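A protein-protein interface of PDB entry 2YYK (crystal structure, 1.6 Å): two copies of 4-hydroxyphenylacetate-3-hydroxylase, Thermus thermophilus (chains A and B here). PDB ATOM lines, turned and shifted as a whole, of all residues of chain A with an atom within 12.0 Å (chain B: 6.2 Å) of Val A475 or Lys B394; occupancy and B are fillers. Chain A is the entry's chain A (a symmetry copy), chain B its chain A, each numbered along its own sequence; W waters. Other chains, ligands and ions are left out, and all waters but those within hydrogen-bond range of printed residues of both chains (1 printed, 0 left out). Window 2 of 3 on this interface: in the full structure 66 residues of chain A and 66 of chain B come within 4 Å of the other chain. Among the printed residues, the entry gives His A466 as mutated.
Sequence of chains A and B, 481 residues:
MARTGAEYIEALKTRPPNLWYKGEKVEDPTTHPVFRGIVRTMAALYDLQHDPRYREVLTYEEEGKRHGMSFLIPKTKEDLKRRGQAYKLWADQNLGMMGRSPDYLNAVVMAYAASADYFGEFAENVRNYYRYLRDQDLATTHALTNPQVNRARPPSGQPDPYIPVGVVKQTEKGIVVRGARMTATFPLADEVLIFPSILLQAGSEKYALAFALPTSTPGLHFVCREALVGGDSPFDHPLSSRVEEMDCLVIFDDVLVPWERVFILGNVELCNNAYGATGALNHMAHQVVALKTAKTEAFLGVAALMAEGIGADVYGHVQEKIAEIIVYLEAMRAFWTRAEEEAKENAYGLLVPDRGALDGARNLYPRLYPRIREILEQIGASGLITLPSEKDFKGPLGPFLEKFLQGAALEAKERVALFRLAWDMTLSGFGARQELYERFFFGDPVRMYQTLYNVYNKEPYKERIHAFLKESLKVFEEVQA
Val A475 touches just these residues of chain B: Pro B234, Phe B235, Glu B390 and Lys B394. Of the printed residues of chain A, Lys B394 touches Val A475 (2.8 Å) and Phe A476 (3.8 Å). No residue of chain A comes within 4 Å of Ser B233. Of chain A, only Ser A472, Val A475 and Phe A476 come within 4 Å of Phe B235. Glu B390 touches two residues of chain A. No residue of chain A comes within 4 Å of Asp B392. No residue of chain A comes within 4 Å of Gly B395. No residue of chain A comes within 4 Å of Pro B396. No residue of chain A comes within 4 Å of Gly B398. Printed residues of chain B within 4 Å of Ser A472: Pro B234 and Phe B235. Of the printed residues of chain B, Glu A471 touches Pro B234 (3.6 Å). Lys A470 touches none of the printed residues of chain B. The nearest residue of chain B that does not touch Val A475 is Ser B233 (4.4 Å).
Of the 12 printed residues of chain A, 4 touch a printed residue of chain B. Hydrophobic or aromatic side chains of chain A that line the printed part of chain B: Val A475 and Phe A476. Printed residues of chain B that touch a printed residue of chain A: Pro B234, Phe B235, Glu B390, Phe B393 and Lys B394. Hydrophobic or aromatic side chains of chain B that line the printed part of chain A: Pro B234, Phe B235 and Phe B393. Among the printed residues, no Asp or Glu carboxylate lies within 4 Å of a Lys or Arg side-chain nitrogen of the other chain.
The side-chain hydroxyl of Ser A472 lies within hydrogen-bond range of the backbone carbonyl oxygen of Pro B234, 3.2 Å away. The side-chain amino group (NZ) of Lys B394 sits at hydrogen-bond distance from the backbone carbonyl oxygen (O) of Val A475, at 2.8 Å.
No position is printed for both chains.
The side-chain hydroxyl (OG) of Ser B233 sits close to the backbone NH (N) of Phe B235, 3.2 Å away. The side-chain hydroxyl (OG) of Ser B233 lies within hydrogen-bond range of the side-chain carboxylate (OE1) of Glu B390 (2.5 Å). The side-chain amino group of Lys B394 lies within salt-bridge range of the side-chain carboxylate of Glu B390 (2.7 Å).
Water W1 lies within hydrogen-bond range of OG of Ser A472 (2.8 Å), O of Phe B235 (2.8 Å) and O of Pro B234 (3.4 Å).
Among the printed residues, pairs that only touch across the chains: Glu A471 with Pro B234, Ser A472 with Phe B235, Val A475 with Pro B234, Val A475 with Phe B235, Val A475 with Glu B390, Phe A476 with Phe B235, Phe A476 with Glu B390, Phe A476 with Phe B393 and Phe A476 with Lys B394.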
ATOM      1  N   HIS A 466     -16.660  36.461 -29.449  1.00  0.00           N
ATOM      2  CA  HIS A 466     -15.498  35.579 -29.429  1.00  0.00           C
ATOM      3  C   HIS A 466     -14.815  35.691 -28.070  1.00  0.00           C
ATOM      4  O   HIS A 466     -14.413  34.693 -27.473  1.00  0.00           O
ATOM      5  CB  HIS A 466     -14.528  35.969 -30.547  1.00  0.00           C
ATOM      6  CG  HIS A 466     -14.791  35.271 -31.847  1.00  0.00           C
ATOM      7  ND1 HIS A 466     -14.376  35.777 -33.061  1.00  0.00           N
ATOM      8  CD2 HIS A 466     -15.384  34.083 -32.120  1.00  0.00           C
ATOM      9  CE1 HIS A 466     -14.701  34.931 -34.023  1.00  0.00           C
ATOM     10  NE2 HIS A 466     -15.314  33.895 -33.479  1.00  0.00           N
ATOM     11  N   ALA A 467     -14.699  36.919 -27.576  1.00  0.00           N
ATOM     12  CA  ALA A 467     -14.077  37.157 -26.281  1.00  0.00           C
ATOM     13  C   ALA A 467     -14.898  36.496 -25.178  1.00  0.00           C
ATOM     14  O   ALA A 467     -14.354  35.863 -24.272  1.00  0.00           O
ATOM     15  CB  ALA A 467     -13.967  38.659 -26.025  1.00  0.00           C
ATOM     16  N   PHE A 468     -16.216  36.627 -25.266  1.00  0.00           N
ATOM     17  CA  PHE A 468     -17.091  36.052 -24.259  1.00  0.00           C
ATOM     18  C   PHE A 468     -17.018  34.530 -24.232  1.00  0.00           C
ATOM     19  O   PHE A 468     -17.168  33.915 -23.175  1.00  0.00           O
ATOM     20  CB  PHE A 468     -18.536  36.507 -24.501  1.00  0.00           C
ATOM     21  CG  PHE A 468     -19.436  36.310 -23.315  1.00  0.00           C
ATOM     22  CD1 PHE A 468     -20.060  35.090 -23.086  1.00  0.00           C
ATOM     23  CD2 PHE A 468     -19.625  37.341 -22.398  1.00  0.00           C
ATOM     24  CE1 PHE A 468     -20.859  34.898 -21.963  1.00  0.00           C
ATOM     25  CE2 PHE A 468     -20.420  37.162 -21.271  1.00  0.00           C
ATOM     26  CZ  PHE A 468     -21.041  35.934 -21.053  1.00  0.00           C
ATOM     27  N   LEU A 469     -16.769  33.930 -25.392  1.00  0.00           N
ATOM     28  CA  LEU A 469     -16.691  32.478 -25.507  1.00  0.00           C
ATOM     29  C   LEU A 469     -15.361  31.879 -25.063  1.00  0.00           C
ATOM     30  O   LEU A 469     -15.220  30.658 -25.026  1.00  0.00           O
ATOM     31  CB  LEU A 469     -16.996  32.047 -26.948  1.00  0.00           C
ATOM     32  CG  LEU A 469     -18.456  32.226 -27.388  1.00  0.00           C
ATOM     33  CD1 LEU A 469     -18.582  31.996 -28.888  1.00  0.00           C
ATOM     34  CD2 LEU A 469     -19.342  31.258 -26.616  1.00  0.00           C
ATOM     35  N   LYS A 470     -14.390  32.721 -24.720  1.00  0.00           N
ATOM     36  CA  LYS A 470     -13.097  32.200 -24.276  1.00  0.00           C
ATOM     37  C   LYS A 470     -13.282  31.308 -23.051  1.00  0.00           C
ATOM     38  O   LYS A 470     -12.664  30.249 -22.949  1.00  0.00           O
ATOM     39  CB  LYS A 470     -12.126  33.339 -23.952  1.00  0.00           C
ATOM     40  CG  LYS A 470     -11.555  34.030 -25.182  1.00  0.00           C
ATOM     41  CD  LYS A 470     -10.558  35.111 -24.794  1.00  0.00           C
ATOM     42  CE  LYS A 470      -9.979  35.793 -26.024  1.00  0.00           C
ATOM     43  NZ  LYS A 470      -9.005  36.861 -25.661  1.00  0.00           N
ATOM     44  N   GLU A 471     -14.142  31.729 -22.128  1.00  0.00           N
ATOM     45  CA  GLU A 471     -14.401  30.944 -20.927  1.00  0.00           C
ATOM     46  C   GLU A 471     -15.044  29.602 -21.257  1.00  0.00           C
ATOM     47  O   GLU A 471     -14.838  28.617 -20.547  1.00  0.00           O
ATOM     48  CB  GLU A 471     -15.293  31.721 -19.954  1.00  0.00           C
ATOM     49  CG  GLU A 471     -14.538  32.704 -19.081  1.00  0.00           C
ATOM     50  CD  GLU A 471     -13.487  32.022 -18.224  1.00  0.00           C
ATOM     51  OE1 GLU A 471     -13.855  31.140 -17.420  1.00  0.00           O
ATOM     52  OE2 GLU A 471     -12.295  32.366 -18.359  1.00  0.00           O
ATOM     53  N   SER A 472     -15.828  29.561 -22.332  1.00  0.00           N
ATOM     54  CA  SER A 472     -16.480  28.320 -22.735  1.00  0.00           C
ATOM     55  C   SER A 472     -15.453  27.291 -23.190  1.00  0.00           C
ATOM     56  O   SER A 472     -15.491  26.138 -22.767  1.00  0.00           O
ATOM     57  CB  SER A 472     -17.468  28.575 -23.879  1.00  0.00           C
ATOM     58  OG  SER A 472     -18.486  29.472 -23.477  1.00  0.00           O
ATOM     59  N   LEU A 473     -14.538  27.712 -24.053  1.00  0.00           N
ATOM     60  CA  LEU A 473     -13.515  26.809 -24.571  1.00  0.00           C
ATOM     61  C   LEU A 473     -12.424  26.487 -23.558  1.00  0.00           C
ATOM     62  O   LEU A 473     -11.685  25.515 -23.724  1.00  0.00           O
ATOM     63  CB  LEU A 473     -12.890  27.402 -25.836  1.00  0.00           C
ATOM     64  CG  LEU A 473     -13.848  27.539 -27.022  1.00  0.00           C
ATOM     65  CD1 LEU A 473     -13.148  28.254 -28.167  1.00  0.00           C
ATOM     66  CD2 LEU A 473     -14.317  26.157 -27.455  1.00  0.00           C
ATOM     67  N   LYS A 474     -12.330  27.292 -22.503  1.00  0.00           N
ATOM     68  CA  LYS A 474     -11.310  27.071 -21.483  1.00  0.00           C
ATOM     69  C   LYS A 474     -11.573  25.824 -20.635  1.00  0.00           C
ATOM     70  O   LYS A 474     -10.663  25.315 -19.977  1.00  0.00           O
ATOM     71  CB  LYS A 474     -11.204  28.297 -20.573  1.00  0.00           C
ATOM     72  CG  LYS A 474     -10.084  28.218 -19.548  1.00  0.00           C
ATOM     73  CD  LYS A 474     -10.043  29.461 -18.673  1.00  0.00           C
ATOM     74  CE  LYS A 474      -8.945  29.360 -17.626  1.00  0.00           C
ATOM     75  NZ  LYS A 474      -8.913  30.551 -16.732  1.00  0.00           N
ATOM     76  N   VAL A 475     -12.806  25.326 -20.651  1.00  0.00           N
ATOM     77  CA  VAL A 475     -13.141  24.143 -19.863  1.00  0.00           C
ATOM     78  C   VAL A 475     -12.361  22.920 -20.334  1.00  0.00           C
ATOM     79  O   VAL A 475     -12.231  21.941 -19.602  1.00  0.00           O
ATOM     80  CB  VAL A 475     -14.654  23.804 -19.936  1.00  0.00           C
ATOM     81  CG1 VAL A 475     -15.483  25.019 -19.537  1.00  0.00           C
ATOM     82  CG2 VAL A 475     -15.024  23.325 -21.335  1.00  0.00           C
ATOM     83  N   PHE A 476     -11.843  22.977 -21.554  1.00  0.00           N
ATOM     84  CA  PHE A 476     -11.097  21.850 -22.099  1.00  0.00           C
ATOM     85  C   PHE A 476      -9.610  21.901 -21.776  1.00  0.00           C
ATOM     86  O   PHE A 476      -8.878  20.953 -22.062  1.00  0.00           O
ATOM     87  CB  PHE A 476     -11.312  21.765 -23.610  1.00  0.00           C
ATOM     88  CG  PHE A 476     -12.751  21.585 -23.997  1.00  0.00           C
ATOM     89  CD1 PHE A 476     -13.452  22.613 -24.619  1.00  0.00           C
ATOM     90  CD2 PHE A 476     -13.417  20.399 -23.704  1.00  0.00           C
ATOM     91  CE1 PHE A 476     -14.799  22.462 -24.945  1.00  0.00           C
ATOM     92  CE2 PHE A 476     -14.765  20.237 -24.025  1.00  0.00           C
ATOM     93  CZ  PHE A 476     -15.458  21.273 -24.647  1.00  0.00           C
ATOM     94  N   GLU A 477      -9.170  23.003 -21.174  1.00  0.00           N
ATOM     95  CA  GLU A 477      -7.767  23.161 -20.802  1.00  0.00           C
ATOM     96  C   GLU A 477      -7.405  22.231 -19.652  1.00  0.00           C
ATOM     97  O   GLU A 477      -8.227  21.970 -18.774  1.00  0.00           O
ATOM     98  CB  GLU A 477      -7.481  24.607 -20.395  1.00  0.00           C
ATOM     99  CG  GLU A 477      -7.241  25.548 -21.561  1.00  0.00           C
ATOM    100  CD  GLU A 477      -6.986  26.975 -21.113  1.00  0.00           C
ATOM    101  OE1 GLU A 477      -6.209  27.168 -20.153  1.00  0.00           O
ATOM    102  OE2 GLU A 477      -7.553  27.902 -21.725  1.00  0.00           O
ATOM    103  N   SER B 233     -21.044  25.142 -15.594  1.00  0.00           N
ATOM    104  CA  SER B 233     -20.170  25.077 -16.760  1.00  0.00           C
ATOM    105  C   SER B 233     -20.389  26.232 -17.725  1.00  0.00           C
ATOM    106  O   SER B 233     -21.503  26.442 -18.209  1.00  0.00           O
ATOM    107  CB  SER B 233     -20.375  23.769 -17.523  1.00  0.00           C
ATOM    108  OG  SER B 233     -19.700  23.827 -18.773  1.00  0.00           O
ATOM    109  N   PRO B 234     -19.326  26.993 -18.019  1.00  0.00           N
ATOM    110  CA  PRO B 234     -19.409  28.129 -18.940  1.00  0.00           C
ATOM    111  C   PRO B 234     -19.713  27.640 -20.357  1.00  0.00           C
ATOM    112  O   PRO B 234     -20.329  28.346 -21.153  1.00  0.00           O
ATOM    113  CB  PRO B 234     -18.019  28.759 -18.842  1.00  0.00           C
ATOM    114  CG  PRO B 234     -17.578  28.401 -17.454  1.00  0.00           C
ATOM    115  CD  PRO B 234     -18.018  26.968 -17.338  1.00  0.00           C
ATOM    116  N   PHE B 235     -19.270  26.425 -20.665  1.00  0.00           N
ATOM    117  CA  PHE B 235     -19.490  25.844 -21.983  1.00  0.00           C
ATOM    118  C   PHE B 235     -20.955  25.452 -22.160  1.00  0.00           C
ATOM    119  O   PHE B 235     -21.588  25.819 -23.148  1.00  0.00           O
ATOM    120  CB  PHE B 235     -18.598  24.608 -22.172  1.00  0.00           C
ATOM    121  CG  PHE B 235     -18.664  24.011 -23.551  1.00  0.00           C
ATOM    122  CD1 PHE B 235     -17.813  24.455 -24.561  1.00  0.00           C
ATOM    123  CD2 PHE B 235     -19.581  23.006 -23.842  1.00  0.00           C
ATOM    124  CE1 PHE B 235     -17.874  23.905 -25.843  1.00  0.00           C
ATOM    125  CE2 PHE B 235     -19.654  22.448 -25.122  1.00  0.00           C
ATOM    126  CZ  PHE B 235     -18.798  22.899 -26.124  1.00  0.00           C
ATOM    127  N   SER B 389     -22.916  18.106 -24.336  1.00  0.00           N
ATOM    128  CA  SER B 389     -22.246  18.781 -23.234  1.00  0.00           C
ATOM    129  C   SER B 389     -20.733  18.709 -23.377  1.00  0.00           C
ATOM    130  O   SER B 389     -20.209  17.906 -24.151  1.00  0.00           O
ATOM    131  CB  SER B 389     -22.655  18.130 -21.910  1.00  0.00           C
ATOM    132  OG  SER B 389     -21.789  18.516 -20.858  1.00  0.00           O
ATOM    133  N   GLU B 390     -20.030  19.556 -22.636  1.00  0.00           N
ATOM    134  CA  GLU B 390     -18.578  19.528 -22.675  1.00  0.00           C
ATOM    135  C   GLU B 390     -18.161  18.139 -22.198  1.00  0.00           C
ATOM    136  O   GLU B 390     -17.115  17.623 -22.591  1.00  0.00           O
ATOM    137  CB  GLU B 390     -17.991  20.594 -21.746  1.00  0.00           C
ATOM    138  CG  GLU B 390     -18.527  20.544 -20.323  1.00  0.00           C
ATOM    139  CD  GLU B 390     -17.534  21.084 -19.310  1.00  0.00           C
ATOM    140  OE1 GLU B 390     -17.735  22.204 -18.790  1.00  0.00           O
ATOM    141  OE2 GLU B 390     -16.541  20.380 -19.037  1.00  0.00           O
ATOM    142  N   LYS B 391     -18.991  17.538 -21.348  1.00  0.00           N
ATOM    143  CA  LYS B 391     -18.710  16.208 -20.812  1.00  0.00           C
ATOM    144  C   LYS B 391     -18.700  15.145 -21.905  1.00  0.00           C
ATOM    145  O   LYS B 391     -18.025  14.123 -21.778  1.00  0.00           O
ATOM    146  CB  LYS B 391     -19.737  15.830 -19.742  1.00  0.00           C
ATOM    147  CG  LYS B 391     -19.698  16.704 -18.497  1.00  0.00           C
ATOM    148  CD  LYS B 391     -20.709  16.217 -17.468  1.00  0.00           C
ATOM    149  CE  LYS B 391     -20.694  17.072 -16.211  1.00  0.00           C
ATOM    150  NZ  LYS B 391     -21.697  16.601 -15.214  1.00  0.00           N
ATOM    151  N   ASP B 392     -19.460  15.369 -22.973  1.00  0.00           N
ATOM    152  CA  ASP B 392     -19.481  14.408 -24.067  1.00  0.00           C
ATOM    153  C   ASP B 392     -18.202  14.537 -24.883  1.00  0.00           C
ATOM    154  O   ASP B 392     -17.682  13.546 -25.392  1.00  0.00           O
ATOM    155  CB  ASP B 392     -20.708  14.621 -24.952  1.00  0.00           C
ATOM    156  CG  ASP B 392     -21.999  14.342 -24.219  1.00  0.00           C
ATOM    157  OD1 ASP B 392     -22.752  15.299 -23.947  1.00  0.00           O
ATOM    158  OD2 ASP B 392     -22.251  13.159 -23.901  1.00  0.00           O
ATOM    159  N   PHE B 393     -17.688  15.759 -25.005  1.00  0.00           N
ATOM    160  CA  PHE B 393     -16.445  15.969 -25.741  1.00  0.00           C
ATOM    161  C   PHE B 393     -15.287  15.366 -24.954  1.00  0.00           C
ATOM    162  O   PHE B 393     -14.319  14.873 -25.533  1.00  0.00           O
ATOM    163  CB  PHE B 393     -16.172  17.462 -25.961  1.00  0.00           C
ATOM    164  CG  PHE B 393     -16.885  18.046 -27.147  1.00  0.00           C
ATOM    165  CD1 PHE B 393     -18.062  18.769 -26.983  1.00  0.00           C
ATOM    166  CD2 PHE B 393     -16.375  17.877 -28.432  1.00  0.00           C
ATOM    167  CE1 PHE B 393     -18.720  19.318 -28.085  1.00  0.00           C
ATOM    168  CE2 PHE B 393     -17.022  18.419 -29.539  1.00  0.00           C
ATOM    169  CZ  PHE B 393     -18.200  19.144 -29.365  1.00  0.00           C
ATOM    170  N   LYS B 394     -15.393  15.413 -23.630  1.00  0.00           N
ATOM    171  CA  LYS B 394     -14.356  14.881 -22.751  1.00  0.00           C
ATOM    172  C   LYS B 394     -14.500  13.377 -22.526  1.00  0.00           C
ATOM    173  O   LYS B 394     -13.590  12.732 -22.001  1.00  0.00           O
ATOM    174  CB  LYS B 394     -14.395  15.596 -21.398  1.00  0.00           C
ATOM    175  CG  LYS B 394     -14.063  17.077 -21.460  1.00  0.00           C
ATOM    176  CD  LYS B 394     -14.169  17.728 -20.089  1.00  0.00           C
ATOM    177  CE  LYS B 394     -13.763  19.195 -20.138  1.00  0.00           C
ATOM    178  NZ  LYS B 394     -13.871  19.853 -18.807  1.00  0.00           N
ATOM    179  N   GLY B 395     -15.642  12.826 -22.925  1.00  0.00           N
ATOM    180  CA  GLY B 395     -15.884  11.406 -22.740  1.00  0.00           C
ATOM    181  C   GLY B 395     -15.377  10.519 -23.864  1.00  0.00           C
ATOM    182  O   GLY B 395     -14.772  11.002 -24.821  1.00  0.00           O
ATOM    183  N   PRO B 396     -15.628   9.205 -23.776  1.00  0.00           N
ATOM    184  CA  PRO B 396     -15.215   8.197 -24.761  1.00  0.00           C
ATOM    185  C   PRO B 396     -15.576   8.505 -26.215  1.00  0.00           C
ATOM    186  O   PRO B 396     -14.847   8.132 -27.133  1.00  0.00           O
ATOM    187  CB  PRO B 396     -15.901   6.928 -24.258  1.00  0.00           C
ATOM    188  CG  PRO B 396     -15.952   7.135 -22.777  1.00  0.00           C
ATOM    189  CD  PRO B 396     -16.383   8.577 -22.677  1.00  0.00           C
ATOM    190  N   LEU B 397     -16.700   9.184 -26.427  1.00  0.00           N
ATOM    191  CA  LEU B 397     -17.136   9.502 -27.781  1.00  0.00           C
ATOM    192  C   LEU B 397     -16.626  10.846 -28.291  1.00  0.00           C
ATOM    193  O   LEU B 397     -16.986  11.272 -29.386  1.00  0.00           O
ATOM    194  CB  LEU B 397     -18.666   9.460 -27.861  1.00  0.00           C
ATOM    195  CG  LEU B 397     -19.303   8.132 -27.439  1.00  0.00           C
ATOM    196  CD1 LEU B 397     -20.815   8.215 -27.574  1.00  0.00           C
ATOM    197  CD2 LEU B 397     -18.754   7.000 -28.297  1.00  0.00           C
ATOM    198  N   GLY B 398     -15.783  11.504 -27.499  1.00  0.00           N
ATOM    199  CA  GLY B 398     -15.239  12.793 -27.895  1.00  0.00           C
ATOM    200  C   GLY B 398     -14.706  12.817 -29.317  1.00  0.00           C
ATOM    201  O   GLY B 398     -15.025  13.727 -30.085  1.00  0.00           O
HETATM  202  O   HOH W   1     -20.711  28.131 -24.555  1.00  0.00           O
